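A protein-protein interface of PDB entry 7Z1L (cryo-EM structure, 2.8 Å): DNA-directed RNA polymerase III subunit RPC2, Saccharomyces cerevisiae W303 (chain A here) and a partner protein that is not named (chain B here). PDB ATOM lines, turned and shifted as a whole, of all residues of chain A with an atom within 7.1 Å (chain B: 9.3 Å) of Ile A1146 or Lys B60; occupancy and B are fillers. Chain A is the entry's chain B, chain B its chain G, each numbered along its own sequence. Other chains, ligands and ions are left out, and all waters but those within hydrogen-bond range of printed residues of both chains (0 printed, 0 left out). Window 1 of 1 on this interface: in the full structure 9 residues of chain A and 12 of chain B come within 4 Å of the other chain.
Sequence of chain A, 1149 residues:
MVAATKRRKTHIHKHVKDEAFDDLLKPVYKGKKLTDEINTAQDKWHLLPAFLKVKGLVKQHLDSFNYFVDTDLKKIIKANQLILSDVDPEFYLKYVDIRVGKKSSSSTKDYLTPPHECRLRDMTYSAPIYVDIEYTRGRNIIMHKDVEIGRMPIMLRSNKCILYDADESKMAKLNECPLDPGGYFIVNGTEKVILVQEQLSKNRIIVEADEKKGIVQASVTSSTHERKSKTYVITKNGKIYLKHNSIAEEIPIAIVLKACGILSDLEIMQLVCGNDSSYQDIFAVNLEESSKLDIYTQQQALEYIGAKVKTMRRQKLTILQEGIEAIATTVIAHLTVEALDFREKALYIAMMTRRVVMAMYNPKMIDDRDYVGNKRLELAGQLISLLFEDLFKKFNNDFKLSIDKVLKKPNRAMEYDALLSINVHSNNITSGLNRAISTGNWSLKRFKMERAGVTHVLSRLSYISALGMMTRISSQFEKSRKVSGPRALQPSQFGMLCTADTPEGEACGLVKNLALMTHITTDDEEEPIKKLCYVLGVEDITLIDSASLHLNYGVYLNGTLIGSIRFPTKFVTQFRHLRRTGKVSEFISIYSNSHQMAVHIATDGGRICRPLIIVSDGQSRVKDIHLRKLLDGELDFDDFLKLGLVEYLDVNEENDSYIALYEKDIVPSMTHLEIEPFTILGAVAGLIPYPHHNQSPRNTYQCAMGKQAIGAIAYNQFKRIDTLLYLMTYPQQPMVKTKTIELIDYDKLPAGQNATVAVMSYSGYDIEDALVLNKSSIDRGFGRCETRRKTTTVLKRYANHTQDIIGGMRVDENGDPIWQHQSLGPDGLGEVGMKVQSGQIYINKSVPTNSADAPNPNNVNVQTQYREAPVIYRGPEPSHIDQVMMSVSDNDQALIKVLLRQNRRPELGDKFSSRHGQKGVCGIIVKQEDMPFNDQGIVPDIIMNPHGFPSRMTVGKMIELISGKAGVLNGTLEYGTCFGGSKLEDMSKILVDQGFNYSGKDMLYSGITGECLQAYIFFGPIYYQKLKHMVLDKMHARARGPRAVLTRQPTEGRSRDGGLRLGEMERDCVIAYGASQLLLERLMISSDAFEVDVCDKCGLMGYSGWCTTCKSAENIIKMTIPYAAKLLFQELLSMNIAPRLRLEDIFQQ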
ATOM      1  N   GLN A1077     -32.948   0.164  -3.000  1.00  0.00           N
ATOM      2  CA  GLN A1077     -31.863   0.187  -2.026  1.00  0.00           C
ATOM      3  C   GLN A1077     -31.518  -1.214  -1.545  1.00  0.00           C
ATOM      4  O   GLN A1077     -30.349  -1.512  -1.284  1.00  0.00           O
ATOM      5  CB  GLN A1077     -32.228   1.087  -0.849  1.00  0.00           C
ATOM      6  CG  GLN A1077     -32.352   2.549  -1.221  1.00  0.00           C
ATOM      7  CD  GLN A1077     -31.099   3.087  -1.872  1.00  0.00           C
ATOM      8  OE1 GLN A1077     -29.994   2.902  -1.364  1.00  0.00           O
ATOM      9  NE2 GLN A1077     -31.261   3.754  -3.007  1.00  0.00           N
ATOM     10  N   GLU A1144     -21.749  12.730 -13.947  1.00  0.00           N
ATOM     11  CA  GLU A1144     -22.545  13.930 -13.750  1.00  0.00           C
ATOM     12  C   GLU A1144     -22.789  14.117 -12.261  1.00  0.00           C
ATOM     13  O   GLU A1144     -22.717  13.165 -11.481  1.00  0.00           O
ATOM     14  CB  GLU A1144     -23.882  13.864 -14.499  1.00  0.00           C
ATOM     15  CG  GLU A1144     -24.873  12.867 -13.924  1.00  0.00           C
ATOM     16  CD  GLU A1144     -26.285  13.094 -14.426  1.00  0.00           C
ATOM     17  OE1 GLU A1144     -26.525  14.127 -15.086  1.00  0.00           O
ATOM     18  OE2 GLU A1144     -27.156  12.239 -14.161  1.00  0.00           O
ATOM     19  N   ASP A1145     -23.064  15.358 -11.873  1.00  0.00           N
ATOM     20  CA  ASP A1145     -23.313  15.661 -10.472  1.00  0.00           C
ATOM     21  C   ASP A1145     -24.651  15.082 -10.034  1.00  0.00           C
ATOM     22  O   ASP A1145     -25.630  15.104 -10.784  1.00  0.00           O
ATOM     23  CB  ASP A1145     -23.290  17.171 -10.245  1.00  0.00           C
ATOM     24  CG  ASP A1145     -21.906  17.763 -10.414  1.00  0.00           C
ATOM     25  OD1 ASP A1145     -20.917  17.043 -10.159  1.00  0.00           O
ATOM     26  OD2 ASP A1145     -21.806  18.945 -10.801  1.00  0.00           O
ATOM     27  N   ILE A1146     -24.685  14.551  -8.810  1.00  0.00           N
ATOM     28  CA  ILE A1146     -25.913  13.955  -8.292  1.00  0.00           C
ATOM     29  C   ILE A1146     -26.960  15.029  -8.033  1.00  0.00           C
ATOM     30  O   ILE A1146     -28.152  14.836  -8.306  1.00  0.00           O
ATOM     31  CB  ILE A1146     -25.612  13.134  -7.026  1.00  0.00           C
ATOM     32  CG1 ILE A1146     -24.583  12.046  -7.333  1.00  0.00           C
ATOM     33  CG2 ILE A1146     -26.881  12.513  -6.469  1.00  0.00           C
ATOM     34  CD1 ILE A1146     -24.284  11.143  -6.164  1.00  0.00           C
ATOM     35  N   PHE A1147     -26.536  16.181  -7.525  1.00  0.00           N
ATOM     36  CA  PHE A1147     -27.443  17.259  -7.159  1.00  0.00           C
ATOM     37  C   PHE A1147     -27.501  18.286  -8.281  1.00  0.00           C
ATOM     38  O   PHE A1147     -26.466  18.665  -8.837  1.00  0.00           O
ATOM     39  CB  PHE A1147     -26.998  17.895  -5.845  1.00  0.00           C
ATOM     40  CG  PHE A1147     -26.794  16.897  -4.747  1.00  0.00           C
ATOM     41  CD1 PHE A1147     -27.868  16.198  -4.226  1.00  0.00           C
ATOM     42  CD2 PHE A1147     -25.528  16.629  -4.260  1.00  0.00           C
ATOM     43  CE1 PHE A1147     -27.688  15.269  -3.229  1.00  0.00           C
ATOM     44  CE2 PHE A1147     -25.343  15.698  -3.261  1.00  0.00           C
ATOM     45  CZ  PHE A1147     -26.425  15.017  -2.747  1.00  0.00           C
ATOM     46  N   GLN A1148     -28.720  18.728  -8.606  1.00  0.00           N
ATOM     47  CA  GLN A1148     -28.949  19.480  -9.837  1.00  0.00           C
ATOM     48  C   GLN A1148     -28.283  20.850  -9.802  1.00  0.00           C
ATOM     49  O   GLN A1148     -27.842  21.354 -10.842  1.00  0.00           O
ATOM     50  CB  GLN A1148     -30.451  19.622 -10.084  1.00  0.00           C
ATOM     51  CG  GLN A1148     -31.142  18.319 -10.450  1.00  0.00           C
ATOM     52  CD  GLN A1148     -32.612  18.508 -10.765  1.00  0.00           C
ATOM     53  OE1 GLN A1148     -33.164  19.592 -10.581  1.00  0.00           O
ATOM     54  NE2 GLN A1148     -33.255  17.449 -11.243  1.00  0.00           N
ATOM     55  N   GLN A1149     -28.214  21.466  -8.620  1.00  0.00           N
ATOM     56  CA  GLN A1149     -27.616  22.792  -8.421  1.00  0.00           C
ATOM     57  C   GLN A1149     -28.265  23.861  -9.297  1.00  0.00           C
ATOM     58  O   GLN A1149     -29.476  24.075  -9.239  1.00  0.00           O
ATOM     59  CB  GLN A1149     -26.105  22.751  -8.678  1.00  0.00           C
ATOM     60  CG  GLN A1149     -25.388  24.058  -8.388  1.00  0.00           C
ATOM     61  CD  GLN A1149     -23.896  23.967  -8.635  1.00  0.00           C
ATOM     62  OE1 GLN A1149     -23.397  22.955  -9.129  1.00  0.00           O
ATOM     63  NE2 GLN A1149     -23.173  25.027  -8.290  1.00  0.00           N
ATOM     64  N   LEU B  10     -21.687  23.579  -2.076  1.00  0.00           N
ATOM     65  CA  LEU B  10     -22.561  22.496  -1.651  1.00  0.00           C
ATOM     66  C   LEU B  10     -22.059  21.975  -0.311  1.00  0.00           C
ATOM     67  O   LEU B  10     -20.966  21.405  -0.236  1.00  0.00           O
ATOM     68  CB  LEU B  10     -22.586  21.379  -2.693  1.00  0.00           C
ATOM     69  CG  LEU B  10     -23.485  20.174  -2.421  1.00  0.00           C
ATOM     70  CD1 LEU B  10     -24.932  20.500  -2.742  1.00  0.00           C
ATOM     71  CD2 LEU B  10     -23.010  18.979  -3.222  1.00  0.00           C
ATOM     72  N   ARG B  12     -22.578  19.701   3.251  1.00  0.00           N
ATOM     73  CA  ARG B  12     -23.187  18.480   3.763  1.00  0.00           C
ATOM     74  C   ARG B  12     -23.382  18.632   5.267  1.00  0.00           C
ATOM     75  O   ARG B  12     -22.410  18.652   6.026  1.00  0.00           O
ATOM     76  CB  ARG B  12     -22.310  17.272   3.440  1.00  0.00           C
ATOM     77  CG  ARG B  12     -22.690  16.004   4.175  1.00  0.00           C
ATOM     78  CD  ARG B  12     -21.773  14.856   3.796  1.00  0.00           C
ATOM     79  NE  ARG B  12     -22.119  13.627   4.499  1.00  0.00           N
ATOM     80  CZ  ARG B  12     -21.714  13.325   5.724  1.00  0.00           C
ATOM     81  NH1 ARG B  12     -20.938  14.141   6.416  1.00  0.00           N
ATOM     82  NH2 ARG B  12     -22.096  12.173   6.268  1.00  0.00           N
ATOM     83  N   GLY B  57     -32.623  21.125   1.126  1.00  0.00           N
ATOM     84  CA  GLY B  57     -31.656  20.085   1.409  1.00  0.00           C
ATOM     85  C   GLY B  57     -31.955  18.787   0.690  1.00  0.00           C
ATOM     86  O   GLY B  57     -32.928  18.101   1.015  1.00  0.00           O
ATOM     87  N   GLN B  58     -31.127  18.440  -0.290  1.00  0.00           N
ATOM     88  CA  GLN B  58     -31.299  17.209  -1.047  1.00  0.00           C
ATOM     89  C   GLN B  58     -30.527  16.081  -0.379  1.00  0.00           C
ATOM     90  O   GLN B  58     -29.467  16.305   0.210  1.00  0.00           O
ATOM     91  CB  GLN B  58     -30.826  17.395  -2.488  1.00  0.00           C
ATOM     92  CG  GLN B  58     -31.252  18.715  -3.101  1.00  0.00           C
ATOM     93  CD  GLN B  58     -30.623  18.961  -4.455  1.00  0.00           C
ATOM     94  OE1 GLN B  58     -30.299  18.023  -5.180  1.00  0.00           O
ATOM     95  NE2 GLN B  58     -30.443  20.229  -4.801  1.00  0.00           N
ATOM     96  N   LEU B  59     -31.065  14.869  -0.468  1.00  0.00           N
ATOM     97  CA  LEU B  59     -30.508  13.713   0.221  1.00  0.00           C
ATOM     98  C   LEU B  59     -30.053  12.670  -0.788  1.00  0.00           C
ATOM     99  O   LEU B  59     -30.801  12.313  -1.703  1.00  0.00           O
ATOM    100  CB  LEU B  59     -31.521  13.098   1.189  1.00  0.00           C
ATOM    101  CG  LEU B  59     -31.714  13.789   2.541  1.00  0.00           C
ATOM    102  CD1 LEU B  59     -32.522  15.062   2.420  1.00  0.00           C
ATOM    103  CD2 LEU B  59     -32.353  12.851   3.534  1.00  0.00           C
ATOM    104  N   LYS B  60     -28.834  12.191  -0.614  1.00  0.00           N
ATOM    105  CA  LYS B  60     -28.257  11.139  -1.436  1.00  0.00           C
ATOM    106  C   LYS B  60     -28.812   9.779  -1.014  1.00  0.00           C
ATOM    107  O   LYS B  60     -28.937   9.505   0.183  1.00  0.00           O
ATOM    108  CB  LYS B  60     -26.737  11.142  -1.303  1.00  0.00           C
ATOM    109  CG  LYS B  60     -26.002  10.485  -2.450  1.00  0.00           C
ATOM    110  CD  LYS B  60     -24.527  10.836  -2.419  1.00  0.00           C
ATOM    111  CE  LYS B  60     -23.832  10.197  -1.235  1.00  0.00           C
ATOM    112  NZ  LYS B  60     -22.384   9.994  -1.500  1.00  0.00           N
ATOM    113  N   PRO B  61     -29.163   8.914  -1.969  1.00  0.00           N
ATOM    114  CA  PRO B  61     -29.579   7.552  -1.608  1.00  0.00           C
ATOM    115  C   PRO B  61     -28.437   6.745  -1.012  1.00  0.00           C
ATOM    116  O   PRO B  61     -27.444   6.463  -1.688  1.00  0.00           O
ATOM    117  CB  PRO B  61     -30.053   6.961  -2.941  1.00  0.00           C
ATOM    118  CG  PRO B  61     -29.403   7.796  -3.988  1.00  0.00           C
ATOM    119  CD  PRO B  61     -29.300   9.171  -3.412  1.00  0.00           C
ATOM    120  N   GLY B  62     -28.571   6.370   0.256  1.00  0.00           N
ATOM    121  CA  GLY B  62     -27.518   5.688   0.976  1.00  0.00           C
ATOM    122  C   GLY B  62     -26.846   6.508   2.053  1.00  0.00           C
ATOM    123  O   GLY B  62     -25.858   6.043   2.633  1.00  0.00           O
ATOM    124  N   ASP B  63     -27.343   7.708   2.340  1.00  0.00           N
ATOM    125  CA  ASP B  63     -26.774   8.560   3.372  1.00  0.00           C
ATOM    126  C   ASP B  63     -27.851   9.523   3.847  1.00  0.00           C
ATOM    127  O   ASP B  63     -28.687   9.964   3.055  1.00  0.00           O
ATOM    128  CB  ASP B  63     -25.554   9.320   2.842  1.00  0.00           C
ATOM    129  CG  ASP B  63     -24.848  10.108   3.917  1.00  0.00           C
ATOM    130  OD1 ASP B  63     -24.158   9.492   4.756  1.00  0.00           O
ATOM    131  OD2 ASP B  63     -24.981  11.347   3.918  1.00  0.00           O
ATOM    132  N   GLY B  64     -27.829   9.843   5.138  1.00  0.00           N
ATOM    133  CA  GLY B  64     -28.882  10.653   5.717  1.00  0.00           C
ATOM    134  C   GLY B  64     -28.566  12.130   5.825  1.00  0.00           C
ATOM    135  O   GLY B  64     -29.455  12.938   6.108  1.00  0.00           O
ATOM    136  N   SER B  65     -27.305  12.494   5.606  1.00  0.00           N
ATOM    137  CA  SER B  65     -26.902  13.890   5.710  1.00  0.00           C
ATOM    138  C   SER B  65     -27.501  14.705   4.575  1.00  0.00           C
ATOM    139  O   SER B  65     -27.586  14.241   3.434  1.00  0.00           O
ATOM    140  CB  SER B  65     -25.379  14.001   5.692  1.00  0.00           C
ATOM    141  OG  SER B  65     -24.855  13.534   4.464  1.00  0.00           O
ATOM    142  N   SER B  66     -27.914  15.929   4.887  1.00  0.00           N
ATOM    143  CA  SER B  66     -28.597  16.774   3.916  1.00  0.00           C
ATOM    144  C   SER B  66     -27.591  17.644   3.177  1.00  0.00           C
ATOM    145  O   SER B  66     -26.759  18.310   3.800  1.00  0.00           O
ATOM    146  CB  SER B  66     -29.645  17.648   4.604  1.00  0.00           C
ATOM    147  OG  SER B  66     -29.033  18.598   5.456  1.00  0.00           O
ATOM    148  N   TYR B  67     -27.674  17.642   1.853  1.00  0.00           N
ATOM    149  CA  TYR B  67     -26.792  18.437   1.010  1.00  0.00           C
ATOM    150  C   TYR B  67     -27.535  19.692   0.575  1.00  0.00           C
ATOM    151  O   TYR B  67     -28.603  19.604  -0.037  1.00  0.00           O
ATOM    152  CB  TYR B  67     -26.326  17.636  -0.204  1.00  0.00           C
ATOM    153  CG  TYR B  67     -25.370  16.510   0.120  1.00  0.00           C
ATOM    154  CD1 TYR B  67     -25.826  15.320   0.667  1.00  0.00           C
ATOM    155  CD2 TYR B  67     -24.013  16.638  -0.127  1.00  0.00           C
ATOM    156  CE1 TYR B  67     -24.956  14.290   0.958  1.00  0.00           C
ATOM    157  CE2 TYR B  67     -23.136  15.615   0.160  1.00  0.00           C
ATOM    158  CZ  TYR B  67     -23.613  14.444   0.703  1.00  0.00           C
ATOM    159  OH  TYR B  67     -22.741  13.422   0.991  1.00  0.00           O
ATOM    160  N   ILE B  68     -26.968  20.854   0.891  1.00  0.00           N
ATOM    161  CA  ILE B  68     -27.602  22.142   0.641  1.00  0.00           C
ATOM    162  C   ILE B  68     -26.708  22.956  -0.282  1.00  0.00           C
ATOM    163  O   ILE B  68     -25.500  23.069  -0.045  1.00  0.00           O
ATOM    164  CB  ILE B  68     -27.868  22.912   1.947  1.00  0.00           C
ATOM    165  CG1 ILE B  68     -28.519  21.998   2.987  1.00  0.00           C
ATOM    166  CG2 ILE B  68     -28.729  24.132   1.676  1.00  0.00           C
ATOM    167  CD1 ILE B  68     -29.057  22.726   4.196  1.00  0.00           C
ATOM    168  N   ASN B  69     -27.301  23.514  -1.334  1.00  0.00           N
ATOM    169  CA  ASN B  69     -26.623  24.482  -2.185  1.00  0.00           C
ATOM    170  C   ASN B  69     -26.792  25.862  -1.566  1.00  0.00           C
ATOM    171  O   ASN B  69     -27.921  26.327  -1.376  1.00  0.00           O
ATOM    172  CB  ASN B  69     -27.189  24.447  -3.603  1.00  0.00           C
ATOM    173  CG  ASN B  69     -26.499  23.424  -4.479  1.00  0.00           C
ATOM    174  OD1 ASN B  69     -25.275  23.411  -4.594  1.00  0.00           O
ATOM    175  ND2 ASN B  69     -27.283  22.548  -5.093  1.00  0.00           N
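The backbone carbonyl oxygen (O) of Gln B58 sits at hydrogen-bond distance from the backbone NH (N) of Tyr B67 (2.8 Å).
Among the printed residues, merely in contact across the chains: Phe A1147 with Gln B58, Gln A1149 with Asn B69, Phe A1147 with Tyr B67, Gln A1077 with Pro B61, Phe A1147 with Leu B10, Ile A1146 with Lys B60 and Gln A1148 with Gln B58.
Of chain B, only Lys B60 (3.8 Å) comes within 4 Å of Ile A1146.
Lys B60 touches just one residue of chain A: Ile A1146.
Phe A1147 touches just these residues of chain B: Leu B10, Gln B58 and Tyr B67.
Of the printed residues of chain A, Asn B69 touches Gln A1149.
Printed residues of chain A within 4 Å of Gln B58: Phe A1147 and Gln A1148.
Of the printed residues of chain B, Gln A1149 touches Asn B69.
Ile B68 touches none of the printed residues of chain A.
The nearest residue of chain B that does not touch Ile A1146 is Gln B58 (5.0 Å).
The nearest residue of chain A that does not touch Lys B60 is Phe A1147 (4.1 Å).
The nearest printed residue of chain A that does not touch Tyr B67 is Ile A1146 (7.6 Å).
Hydrophobic or aromatic side chains of chain A that line the printed part of chain B: Ile A1146 and Phe A1147.
Of the 15 printed residues of chain B, 6 touch a printed residue of chain A.
Hydrophobic or aromatic side chains of chain B that line the printed part of chain A: Leu B10, Pro B61 and Tyr B67.
Among the printed residues, 7 pairs touch across the chains.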
